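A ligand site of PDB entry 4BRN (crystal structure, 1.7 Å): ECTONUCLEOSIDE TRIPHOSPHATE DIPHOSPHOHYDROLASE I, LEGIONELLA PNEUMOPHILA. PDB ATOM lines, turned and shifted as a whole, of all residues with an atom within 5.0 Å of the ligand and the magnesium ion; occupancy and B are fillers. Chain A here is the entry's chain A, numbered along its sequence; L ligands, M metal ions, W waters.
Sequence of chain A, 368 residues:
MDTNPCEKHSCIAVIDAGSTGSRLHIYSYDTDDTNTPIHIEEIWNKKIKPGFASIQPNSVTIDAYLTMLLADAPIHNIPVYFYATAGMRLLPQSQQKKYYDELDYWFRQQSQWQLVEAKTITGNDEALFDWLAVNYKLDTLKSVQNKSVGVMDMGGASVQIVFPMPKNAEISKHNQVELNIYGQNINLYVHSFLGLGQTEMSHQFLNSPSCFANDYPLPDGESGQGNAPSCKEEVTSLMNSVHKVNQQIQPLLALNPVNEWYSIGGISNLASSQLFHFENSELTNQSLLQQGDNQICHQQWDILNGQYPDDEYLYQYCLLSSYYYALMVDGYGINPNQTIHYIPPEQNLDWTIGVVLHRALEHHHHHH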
ATOM      1  N   ASP A  16      -8.000  -6.484  -2.107  1.00  0.00           N
ATOM      2  CA  ASP A  16      -7.042  -6.094  -3.142  1.00  0.00           C
ATOM      3  C   ASP A  16      -7.339  -4.663  -3.549  1.00  0.00           C
ATOM      4  O   ASP A  16      -8.311  -4.381  -4.262  1.00  0.00           O
ATOM      5  CB  ASP A  16      -7.254  -7.059  -4.318  1.00  0.00           C
ATOM      6  CG  ASP A  16      -6.634  -6.577  -5.614  1.00  0.00           C
ATOM      7  OD1 ASP A  16      -5.801  -5.621  -5.590  1.00  0.00           O
ATOM      8  OD2 ASP A  16      -6.938  -7.175  -6.687  1.00  0.00           O
ATOM      9  N   GLY A  18      -6.244  -2.420  -5.897  1.00  0.00           N
ATOM     10  CA  GLY A  18      -5.532  -2.194  -7.133  1.00  0.00           C
ATOM     11  C   GLY A  18      -5.627  -0.779  -7.609  1.00  0.00           C
ATOM     12  O   GLY A  18      -6.307   0.089  -7.043  1.00  0.00           O
ATOM     13  N   SER A  19      -4.979  -0.530  -8.757  1.00  0.00           N
ATOM     14  CA  SER A  19      -4.884   0.858  -9.234  1.00  0.00           C
ATOM     15  C   SER A  19      -6.220   1.387  -9.786  1.00  0.00           C
ATOM     16  O   SER A  19      -6.454   2.613  -9.761  1.00  0.00           O
ATOM     17  CB  SER A  19      -3.719   1.056 -10.238  1.00  0.00           C
ATOM     18  OG  SER A  19      -4.023   0.530 -11.495  1.00  0.00           O
ATOM     19  N   THR A  20      -7.093   0.456 -10.230  1.00  0.00           N
ATOM     20  CA  THR A  20      -8.327   0.869 -10.835  1.00  0.00           C
ATOM     21  C   THR A  20      -9.580   0.595  -9.965  1.00  0.00           C
ATOM     22  O   THR A  20     -10.688   1.004 -10.344  1.00  0.00           O
ATOM     23  CB  THR A  20      -8.460   0.213 -12.279  1.00  0.00           C
ATOM     24  OG1 THR A  20      -8.596  -1.256 -12.189  1.00  0.00           O
ATOM     25  CG2 THR A  20      -7.159   0.629 -13.131  1.00  0.00           C
ATOM     26  N   GLY A  21      -9.439  -0.092  -8.838  1.00  0.00           N
ATOM     27  CA  GLY A  21     -10.602  -0.474  -8.038  1.00  0.00           C
ATOM     28  C   GLY A  21     -10.110  -1.271  -6.856  1.00  0.00           C
ATOM     29  O   GLY A  21      -8.936  -1.758  -6.843  1.00  0.00           O
ATOM     30  N   ARG A  23     -11.209  -4.730  -4.471  1.00  0.00           N
ATOM     31  CA  ARG A  23     -12.103  -5.881  -4.442  1.00  0.00           C
ATOM     32  C   ARG A  23     -11.955  -6.509  -3.060  1.00  0.00           C
ATOM     33  O   ARG A  23     -10.861  -6.900  -2.613  1.00  0.00           O
ATOM     34  CB  ARG A  23     -11.787  -6.890  -5.527  1.00  0.00           C
ATOM     35  CG  ARG A  23     -11.614  -6.238  -6.885  1.00  0.00           C
ATOM     36  CD  ARG A  23     -10.124  -5.909  -7.180  1.00  0.00           C
ATOM     37  NE  ARG A  23     -10.124  -4.945  -8.342  1.00  0.00           N
ATOM     38  CZ  ARG A  23      -9.017  -4.501  -8.925  1.00  0.00           C
ATOM     39  NH1 ARG A  23      -7.841  -4.954  -8.499  1.00  0.00           N
ATOM     40  NH2 ARG A  23      -9.093  -3.599  -9.928  1.00  0.00           N
ATOM     41  N   THR A  85      -1.622  -2.174  -4.094  1.00  0.00           N
ATOM     42  CA  THR A  85      -0.554  -2.457  -5.000  1.00  0.00           C
ATOM     43  C   THR A  85      -0.032  -1.151  -5.720  1.00  0.00           C
ATOM     44  O   THR A  85       0.245  -0.122  -5.067  1.00  0.00           O
ATOM     45  CB  THR A  85      -0.944  -3.648  -5.913  1.00  0.00           C
ATOM     46  OG1 THR A  85      -2.099  -3.312  -6.689  1.00  0.00           O
ATOM     47  CG2 THR A  85      -1.266  -4.896  -5.083  1.00  0.00           C
ATOM     48  N   GLU A 126       3.523  -8.887  -4.461  1.00  0.00           N
ATOM     49  CA  GLU A 126       2.341  -9.090  -5.329  1.00  0.00           C
ATOM     50  C   GLU A 126       2.577 -10.232  -6.332  1.00  0.00           C
ATOM     51  O   GLU A 126       1.659 -11.008  -6.558  1.00  0.00           O
ATOM     52  CB  GLU A 126       2.064  -7.780  -6.056  1.00  0.00           C
ATOM     53  CG  GLU A 126       0.769  -7.699  -6.882  1.00  0.00           C
ATOM     54  CD  GLU A 126       0.631  -6.324  -7.523  1.00  0.00           C
ATOM     55  OE1 GLU A 126       1.568  -5.462  -7.362  1.00  0.00           O
ATOM     56  OE2 GLU A 126      -0.401  -6.040  -8.192  1.00  0.00           O
ATOM     57  N   ASP A 153       0.524 -10.986 -14.341  1.00  0.00           N
ATOM     58  CA  ASP A 153      -0.594 -10.200 -13.835  1.00  0.00           C
ATOM     59  C   ASP A 153      -0.499  -8.817 -14.507  1.00  0.00           C
ATOM     60  O   ASP A 153       0.469  -8.092 -14.328  1.00  0.00           O
ATOM     61  CB  ASP A 153      -0.492 -10.092 -12.299  1.00  0.00           C
ATOM     62  CG  ASP A 153      -1.576  -9.219 -11.705  1.00  0.00           C
ATOM     63  OD1 ASP A 153      -2.071  -8.287 -12.402  1.00  0.00           O
ATOM     64  OD2 ASP A 153      -1.877  -9.332 -10.480  1.00  0.00           O
ATOM     65  N   MET A 154      -1.502  -8.536 -15.343  1.00  0.00           N
ATOM     66  CA  MET A 154      -1.627  -7.265 -16.105  1.00  0.00           C
ATOM     67  C   MET A 154      -2.475  -6.254 -15.340  1.00  0.00           C
ATOM     68  O   MET A 154      -3.714  -6.297 -15.395  1.00  0.00           O
ATOM     69  CB  MET A 154      -2.279  -7.569 -17.479  1.00  0.00           C
ATOM     70  CG  MET A 154      -1.661  -8.784 -18.153  1.00  0.00           C
ATOM     71  SD  MET A 154       0.057  -8.422 -18.557  1.00  0.00           S
ATOM     72  CE  MET A 154       0.487  -9.863 -19.556  1.00  0.00           C
ATOM     73  N   GLY A 155      -1.819  -5.364 -14.589  1.00  0.00           N
ATOM     74  CA  GLY A 155      -2.609  -4.382 -13.810  1.00  0.00           C
ATOM     75  C   GLY A 155      -2.571  -2.981 -14.413  1.00  0.00           C
ATOM     76  O   GLY A 155      -2.039  -2.765 -15.531  1.00  0.00           O
ATOM     77  N   GLY A 156      -3.119  -2.061 -13.685  1.00  0.00           N
ATOM     78  CA  GLY A 156      -3.374  -0.670 -14.228  1.00  0.00           C
ATOM     79  C   GLY A 156      -2.089   0.144 -14.149  1.00  0.00           C
ATOM     80  O   GLY A 156      -1.858   1.028 -15.003  1.00  0.00           O
ATOM     81  N   ALA A 157      -1.243  -0.091 -13.121  1.00  0.00           N
ATOM     82  CA  ALA A 157      -0.065   0.723 -12.912  1.00  0.00           C
ATOM     83  C   ALA A 157       1.229  -0.124 -12.946  1.00  0.00           C
ATOM     84  O   ALA A 157       2.279   0.386 -13.254  1.00  0.00           O
ATOM     85  CB  ALA A 157      -0.107   1.493 -11.582  1.00  0.00           C
ATOM     86  N   GLN A 198      -1.498  -0.837 -17.515  1.00  0.00           N
ATOM     87  CA  GLN A 198      -2.296  -0.344 -18.654  1.00  0.00           C
ATOM     88  C   GLN A 198      -2.543   1.147 -18.625  1.00  0.00           C
ATOM     89  O   GLN A 198      -2.392   1.797 -19.656  1.00  0.00           O
ATOM     90  CB  GLN A 198      -3.662  -1.031 -18.617  1.00  0.00           C
ATOM     91  CG  GLN A 198      -4.558  -0.675 -19.754  1.00  0.00           C
ATOM     92  CD  GLN A 198      -5.831  -1.504 -19.705  1.00  0.00           C
ATOM     93  OE1 GLN A 198      -5.788  -2.745 -19.560  1.00  0.00           O
ATOM     94  NE2 GLN A 198      -6.971  -0.836 -19.854  1.00  0.00           N
ATOM     95  N   THR A 199      -2.943   1.695 -17.483  1.00  0.00           N
ATOM     96  CA  THR A 199      -3.286   3.110 -17.414  1.00  0.00           C
ATOM     97  C   THR A 199      -2.037   3.932 -17.606  1.00  0.00           C
ATOM     98  O   THR A 199      -2.046   4.896 -18.413  1.00  0.00           O
ATOM     99  CB  THR A 199      -3.871   3.475 -16.004  1.00  0.00           C
ATOM    100  OG1 THR A 199      -4.911   2.567 -15.690  1.00  0.00           O
ATOM    101  CG2 THR A 199      -4.432   4.915 -15.934  1.00  0.00           C
ATOM    102  N   GLY A 265      -5.680 -10.388 -14.722  1.00  0.00           N
ATOM    103  CA  GLY A 265      -5.765  -8.886 -14.863  1.00  0.00           C
ATOM    104  C   GLY A 265      -6.504  -8.531 -16.137  1.00  0.00           C
ATOM    105  O   GLY A 265      -7.364  -9.322 -16.598  1.00  0.00           O
ATOM    106  N   GLY A 266      -6.141  -7.375 -16.698  1.00  0.00           N
ATOM    107  CA  GLY A 266      -6.956  -6.683 -17.717  1.00  0.00           C
ATOM    108  C   GLY A 266      -7.053  -7.524 -18.980  1.00  0.00           C
ATOM    109  O   GLY A 266      -8.026  -7.397 -19.729  1.00  0.00           O
ATOM    110  N   ASN A 269     -10.134  -9.617 -19.239  1.00  0.00           N
ATOM    111  CA  ASN A 269     -11.278  -8.856 -19.708  1.00  0.00           C
ATOM    112  C   ASN A 269     -11.217  -8.635 -21.219  1.00  0.00           C
ATOM    113  O   ASN A 269     -12.229  -8.885 -21.916  1.00  0.00           O
ATOM    114  CB  ASN A 269     -11.405  -7.544 -18.954  1.00  0.00           C
ATOM    115  CG  ASN A 269     -11.404  -7.746 -17.447  1.00  0.00           C
ATOM    116  OD1 ASN A 269     -10.348  -7.691 -16.828  1.00  0.00           O
ATOM    117  ND2 ASN A 269     -12.570  -8.009 -16.856  1.00  0.00           N
ATOM    118  N   LEU A 270     -10.069  -8.179 -21.717  1.00  0.00           N
ATOM    119  CA  LEU A 270      -9.933  -7.931 -23.177  1.00  0.00           C
ATOM    120  C   LEU A 270     -10.279  -9.171 -23.991  1.00  0.00           C
ATOM    121  O   LEU A 270     -11.116  -9.093 -24.924  1.00  0.00           O
ATOM    122  CB  LEU A 270      -8.519  -7.487 -23.542  1.00  0.00           C
ATOM    123  CG  LEU A 270      -8.283  -7.093 -25.007  1.00  0.00           C
ATOM    124  CD1 LEU A 270      -9.145  -5.884 -25.333  1.00  0.00           C
ATOM    125  CD2 LEU A 270      -6.786  -6.772 -25.335  1.00  0.00           C
ATOM    126  N   TYR A 313     -14.056   0.188 -22.042  1.00  0.00           N
ATOM    127  CA  TYR A 313     -12.693   0.054 -22.460  1.00  0.00           C
ATOM    128  C   TYR A 313     -12.437   0.015 -23.969  1.00  0.00           C
ATOM    129  O   TYR A 313     -11.298   0.104 -24.389  1.00  0.00           O
ATOM    130  CB  TYR A 313     -12.089  -1.181 -21.801  1.00  0.00           C
ATOM    131  CG  TYR A 313     -11.638  -0.900 -20.385  1.00  0.00           C
ATOM    132  CD1 TYR A 313     -10.347  -0.389 -20.120  1.00  0.00           C
ATOM    133  CD2 TYR A 313     -12.486  -1.157 -19.309  1.00  0.00           C
ATOM    134  CE1 TYR A 313      -9.912  -0.178 -18.796  1.00  0.00           C
ATOM    135  CE2 TYR A 313     -12.059  -0.915 -17.993  1.00  0.00           C
ATOM    136  CZ  TYR A 313     -10.790  -0.445 -17.746  1.00  0.00           C
ATOM    137  OH  TYR A 313     -10.393  -0.207 -16.429  1.00  0.00           O
ATOM    138  N   TYR A 317      -8.910  -0.687 -27.173  1.00  0.00           N
ATOM    139  CA  TYR A 317      -8.597  -2.095 -27.505  1.00  0.00           C
ATOM    140  C   TYR A 317      -7.504  -2.277 -28.537  1.00  0.00           C
ATOM    141  O   TYR A 317      -6.875  -3.324 -28.575  1.00  0.00           O
ATOM    142  CB  TYR A 317      -9.865  -2.841 -27.991  1.00  0.00           C
ATOM    143  CG  TYR A 317     -10.808  -3.253 -26.901  1.00  0.00           C
ATOM    144  CD1 TYR A 317     -10.616  -2.911 -25.542  1.00  0.00           C
ATOM    145  CD2 TYR A 317     -11.969  -3.937 -27.256  1.00  0.00           C
ATOM    146  CE1 TYR A 317     -11.540  -3.322 -24.568  1.00  0.00           C
ATOM    147  CE2 TYR A 317     -12.896  -4.336 -26.321  1.00  0.00           C
ATOM    148  CZ  TYR A 317     -12.682  -4.038 -24.996  1.00  0.00           C
ATOM    149  OH  TYR A 317     -13.699  -4.447 -24.182  1.00  0.00           O
ATOM    150  N   LEU A 320      -4.383  -1.652 -26.511  1.00  0.00           N
ATOM    151  CA  LEU A 320      -4.216  -2.810 -25.586  1.00  0.00           C
ATOM    152  C   LEU A 320      -3.686  -4.076 -26.285  1.00  0.00           C
ATOM    153  O   LEU A 320      -2.777  -4.738 -25.774  1.00  0.00           O
ATOM    154  CB  LEU A 320      -5.456  -3.056 -24.716  1.00  0.00           C
ATOM    155  CG  LEU A 320      -5.912  -1.888 -23.835  1.00  0.00           C
ATOM    156  CD1 LEU A 320      -7.210  -2.371 -23.177  1.00  0.00           C
ATOM    157  CD2 LEU A 320      -4.832  -1.542 -22.804  1.00  0.00           C
ATOM    158  N   TYR A 324      -0.118  -5.551 -25.235  1.00  0.00           N
ATOM    159  CA  TYR A 324       0.110  -6.898 -24.709  1.00  0.00           C
ATOM    160  C   TYR A 324       1.184  -7.646 -25.492  1.00  0.00           C
ATOM    161  O   TYR A 324       1.988  -8.384 -24.905  1.00  0.00           O
ATOM    162  CB  TYR A 324      -1.159  -7.737 -24.607  1.00  0.00           C
ATOM    163  CG  TYR A 324      -2.068  -7.296 -23.513  1.00  0.00           C
ATOM    164  CD1 TYR A 324      -1.583  -7.121 -22.166  1.00  0.00           C
ATOM    165  CD2 TYR A 324      -3.407  -7.053 -23.773  1.00  0.00           C
ATOM    166  CE1 TYR A 324      -2.465  -6.705 -21.153  1.00  0.00           C
ATOM    167  CE2 TYR A 324      -4.278  -6.623 -22.784  1.00  0.00           C
ATOM    168  CZ  TYR A 324      -3.810  -6.440 -21.505  1.00  0.00           C
ATOM    169  OH  TYR A 324      -4.759  -6.027 -20.607  1.00  0.00           O
ATOM    170  N   TRP A 351      -4.684 -12.026  -6.757  1.00  0.00           N
ATOM    171  CA  TRP A 351      -3.638 -12.625  -5.992  1.00  0.00           C
ATOM    172  C   TRP A 351      -4.089 -12.856  -4.507  1.00  0.00           C
ATOM    173  O   TRP A 351      -3.285 -13.321  -3.694  1.00  0.00           O
ATOM    174  CB  TRP A 351      -2.420 -11.696  -6.020  1.00  0.00           C
ATOM    175  CG  TRP A 351      -2.787 -10.266  -5.817  1.00  0.00           C
ATOM    176  CD1 TRP A 351      -3.036  -9.358  -6.807  1.00  0.00           C
ATOM    177  CD2 TRP A 351      -3.006  -9.578  -4.591  1.00  0.00           C
ATOM    178  NE1 TRP A 351      -3.348  -8.126  -6.289  1.00  0.00           N
ATOM    179  CE2 TRP A 351      -3.336  -8.228  -4.922  1.00  0.00           C
ATOM    180  CE3 TRP A 351      -2.917  -9.956  -3.218  1.00  0.00           C
ATOM    181  CZ2 TRP A 351      -3.612  -7.271  -3.984  1.00  0.00           C
ATOM    182  CZ3 TRP A 351      -3.144  -8.966  -2.273  1.00  0.00           C
ATOM    183  CH2 TRP A 351      -3.554  -7.634  -2.664  1.00  0.00           C
HETATM  184  P1  LIG L   1      -5.578  -3.262 -10.979  1.00  0.00           P
HETATM  185  O1  LIG L   1      -6.798  -2.412 -10.822  1.00  0.00           O
HETATM  186  O2  LIG L   1      -4.208  -2.559 -10.852  1.00  0.00           O
HETATM  187  O3  LIG L   1      -5.725  -4.498 -10.123  1.00  0.00           O
HETATM  188  O4  LIG L   1      -5.532  -3.799 -12.516  1.00  0.00           O
HETATM  189  C1  LIG L   1      -6.682  -4.354 -13.207  1.00  0.00           C
HETATM  190  C2  LIG L   1      -6.444  -4.026 -14.685  1.00  0.00           C
HETATM  191  O5  LIG L   1      -7.613  -4.573 -15.400  1.00  0.00           O
HETATM  192  C3  LIG L   1      -6.441  -2.537 -14.939  1.00  0.00           C
HETATM  193  O6  LIG L   1      -5.506  -2.119 -15.966  1.00  0.00           O
HETATM  194  C4  LIG L   1      -7.845  -2.294 -15.527  1.00  0.00           C
HETATM  195  O7  LIG L   1      -7.930  -1.082 -16.282  1.00  0.00           O
HETATM  196  C5  LIG L   1      -7.959  -3.561 -16.341  1.00  0.00           C
HETATM  197  N1  LIG L   1      -9.338  -3.788 -16.768  1.00  0.00           N
HETATM  198  C6  LIG L   1     -10.426  -3.814 -15.942  1.00  0.00           C
HETATM  199  N2  LIG L   1     -11.530  -4.008 -16.746  1.00  0.00           N
HETATM  200  C7  LIG L   1     -11.105  -4.156 -17.997  1.00  0.00           C
HETATM  201  C8  LIG L   1     -11.795  -4.338 -19.283  1.00  0.00           C
HETATM  202  N3  LIG L   1     -13.139  -4.492 -19.233  1.00  0.00           N
HETATM  203  N4  LIG L   1     -11.016  -4.438 -20.378  1.00  0.00           N
HETATM  204  C9  LIG L   1      -9.671  -4.274 -20.387  1.00  0.00           C
HETATM  205  N5  LIG L   1      -8.973  -4.042 -19.235  1.00  0.00           N
HETATM  206  C10 LIG L   1      -9.670  -3.980 -18.052  1.00  0.00           C
HETATM  207 MG    MG M   1      -4.151  -5.921  -9.557  1.00  0.00          MG
HETATM  208  O   HOH W   1      -2.747  -4.488  -9.951  1.00  0.00           O
HETATM  209  O   HOH W   2      -6.246   1.113 -17.071  1.00  0.00           O
HETATM  210  O   HOH W   3      -4.624  -4.400 -17.786  1.00  0.00           O
HETATM  211  O   HOH W   4      -5.685  -7.346  -8.970  1.00  0.00           O
HETATM  212  O   HOH W   5      -4.192  -6.858 -11.539  1.00  0.00           O
HETATM  213  O   HOH W   6      -1.610  -1.835 -10.869  1.00  0.00           O
HETATM  214  O   HOH W   7      -4.118  -5.231  -7.518  1.00  0.00           O
HETATM  215  O   HOH W   8     -13.880  -4.032 -15.092  1.00  0.00           O
HETATM  216  O   HOH W   9      -2.599  -7.226  -9.128  1.00  0.00           O
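O1 of the ligand sits at hydrogen-bond distance from OG1 of Thr 20, 2.5 Å away.
An oxygen (O2) of the ligand sits at hydrogen-bond distance from the backbone NH (N) of Ser 19 (3.0 Å).
An oxygen (O1) of the ligand is in salt-bridge range of the guanidinium group of Arg 23, at 2.7 Å.
The backbone NH (N) of Gly 156 is in hydrogen-bond range of an oxygen (O2) of the ligand, 3.1 Å away.
An oxygen (O2) of the ligand is in hydrogen-bond range of the side-chain hydroxyl (OG) of Ser 19 (3.2 Å).
O1 of the ligand lies within hydrogen-bond range of N of Thr 20.
OE1 of Gln 198 sits close to N5 of the ligand (3.5 Å).
N of Gly 266 lies close to O5 of the ligand, at 3.4 Å.
The side-chain hydroxyl (OH) of Tyr 313 lies within hydrogen-bond range of an oxygen (O7) of the ligand, 2.6 Å away.
The backbone carbonyl oxygen (O) of Gly 155 is in hydrogen-bond range of the backbone NH (N) of Gln 198.
The backbone NH of Gly 18 is in hydrogen-bond range of the side-chain carboxylate of Asp 16, 3.2 Å away.
The side-chain amide oxygen (OD1) of Asn 269 sits close to the backbone carbonyl oxygen (O) of Gly 265 (3.4 Å).
OG of Ser 19 sits at hydrogen-bond distance from N of Ala 157, 3.3 Å away.
The backbone carbonyl oxygen of Met 154 is in hydrogen-bond range of the backbone NH of Gly 266 (3.0 Å).
The backbone NH (N) of Thr 199 lies within hydrogen-bond range of the backbone carbonyl oxygen (O) of Gly 156 (2.8 Å).
OD2 of Asp 16 is in salt-bridge range of NH1 of Arg 23 (3.0 Å).
OG1 of Thr 20 is in hydrogen-bond range of NH2 of Arg 23 (3.3 Å).
Residues that only touch the ligand: Gly 18 (3.8 Å), Met 154 (3.6 Å), Gly 155 (3.2 Å) and Asn 269 (3.2 Å).
Hydrophobic or aromatic side chains that line the ligand: Tyr 313.
Of the 24 residues printed, 11 come within 4 Å of the ligand.
The nearest printed residue that does not touch the ligand is Gly 21 (4.04 Å).
Arg 23 touches the magnesium ion (NH1 to MG, 3.96 Å).
OE2 of Glu 126 touches the magnesium ion (3.99 Å).
Of the 24 residues printed, 2 come within 4 Å of the magnesium ion.
The magnesium ion is bound by water W1, water W9, water W7, water W4, water W5 and an oxygen (O3) of the ligand.
Water W1 lies within hydrogen-bond range of an oxygen (O2) of the ligand and the side-chain carboxylate (OE2) of Glu 126.
Water W5 lies within hydrogen-bond range of OD1 of Asp 153 and O4 of the ligand.
Water W7 lies within hydrogen-bond range of OD1 of Asp 16 (2.6 Å), OG1 of Thr 85 (2.9 Å) and NE1 of Trp 351 (3.2 Å).
Water W4 lies within hydrogen-bond range of the side-chain carboxylate of Asp 16 (2.6 Å) and the guanidinium group of Arg 23 (3.3 Å).
Water W9 lies within hydrogen-bond range of the side-chain carboxylate (OD2) of Asp 153 (2.6 Å), the side-chain carboxylate (OE2) of Glu 126 (2.7 Å) and the indole nitrogen (NE1) of Trp 351 (3.1 Å).
Water W3 lies within hydrogen-bond range of OE1 of Gln 198 (2.7 Å), O6 of the ligand (3.0 Å), O of Met 154 (3.2 Å) and OH of Tyr 324 (3.3 Å).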
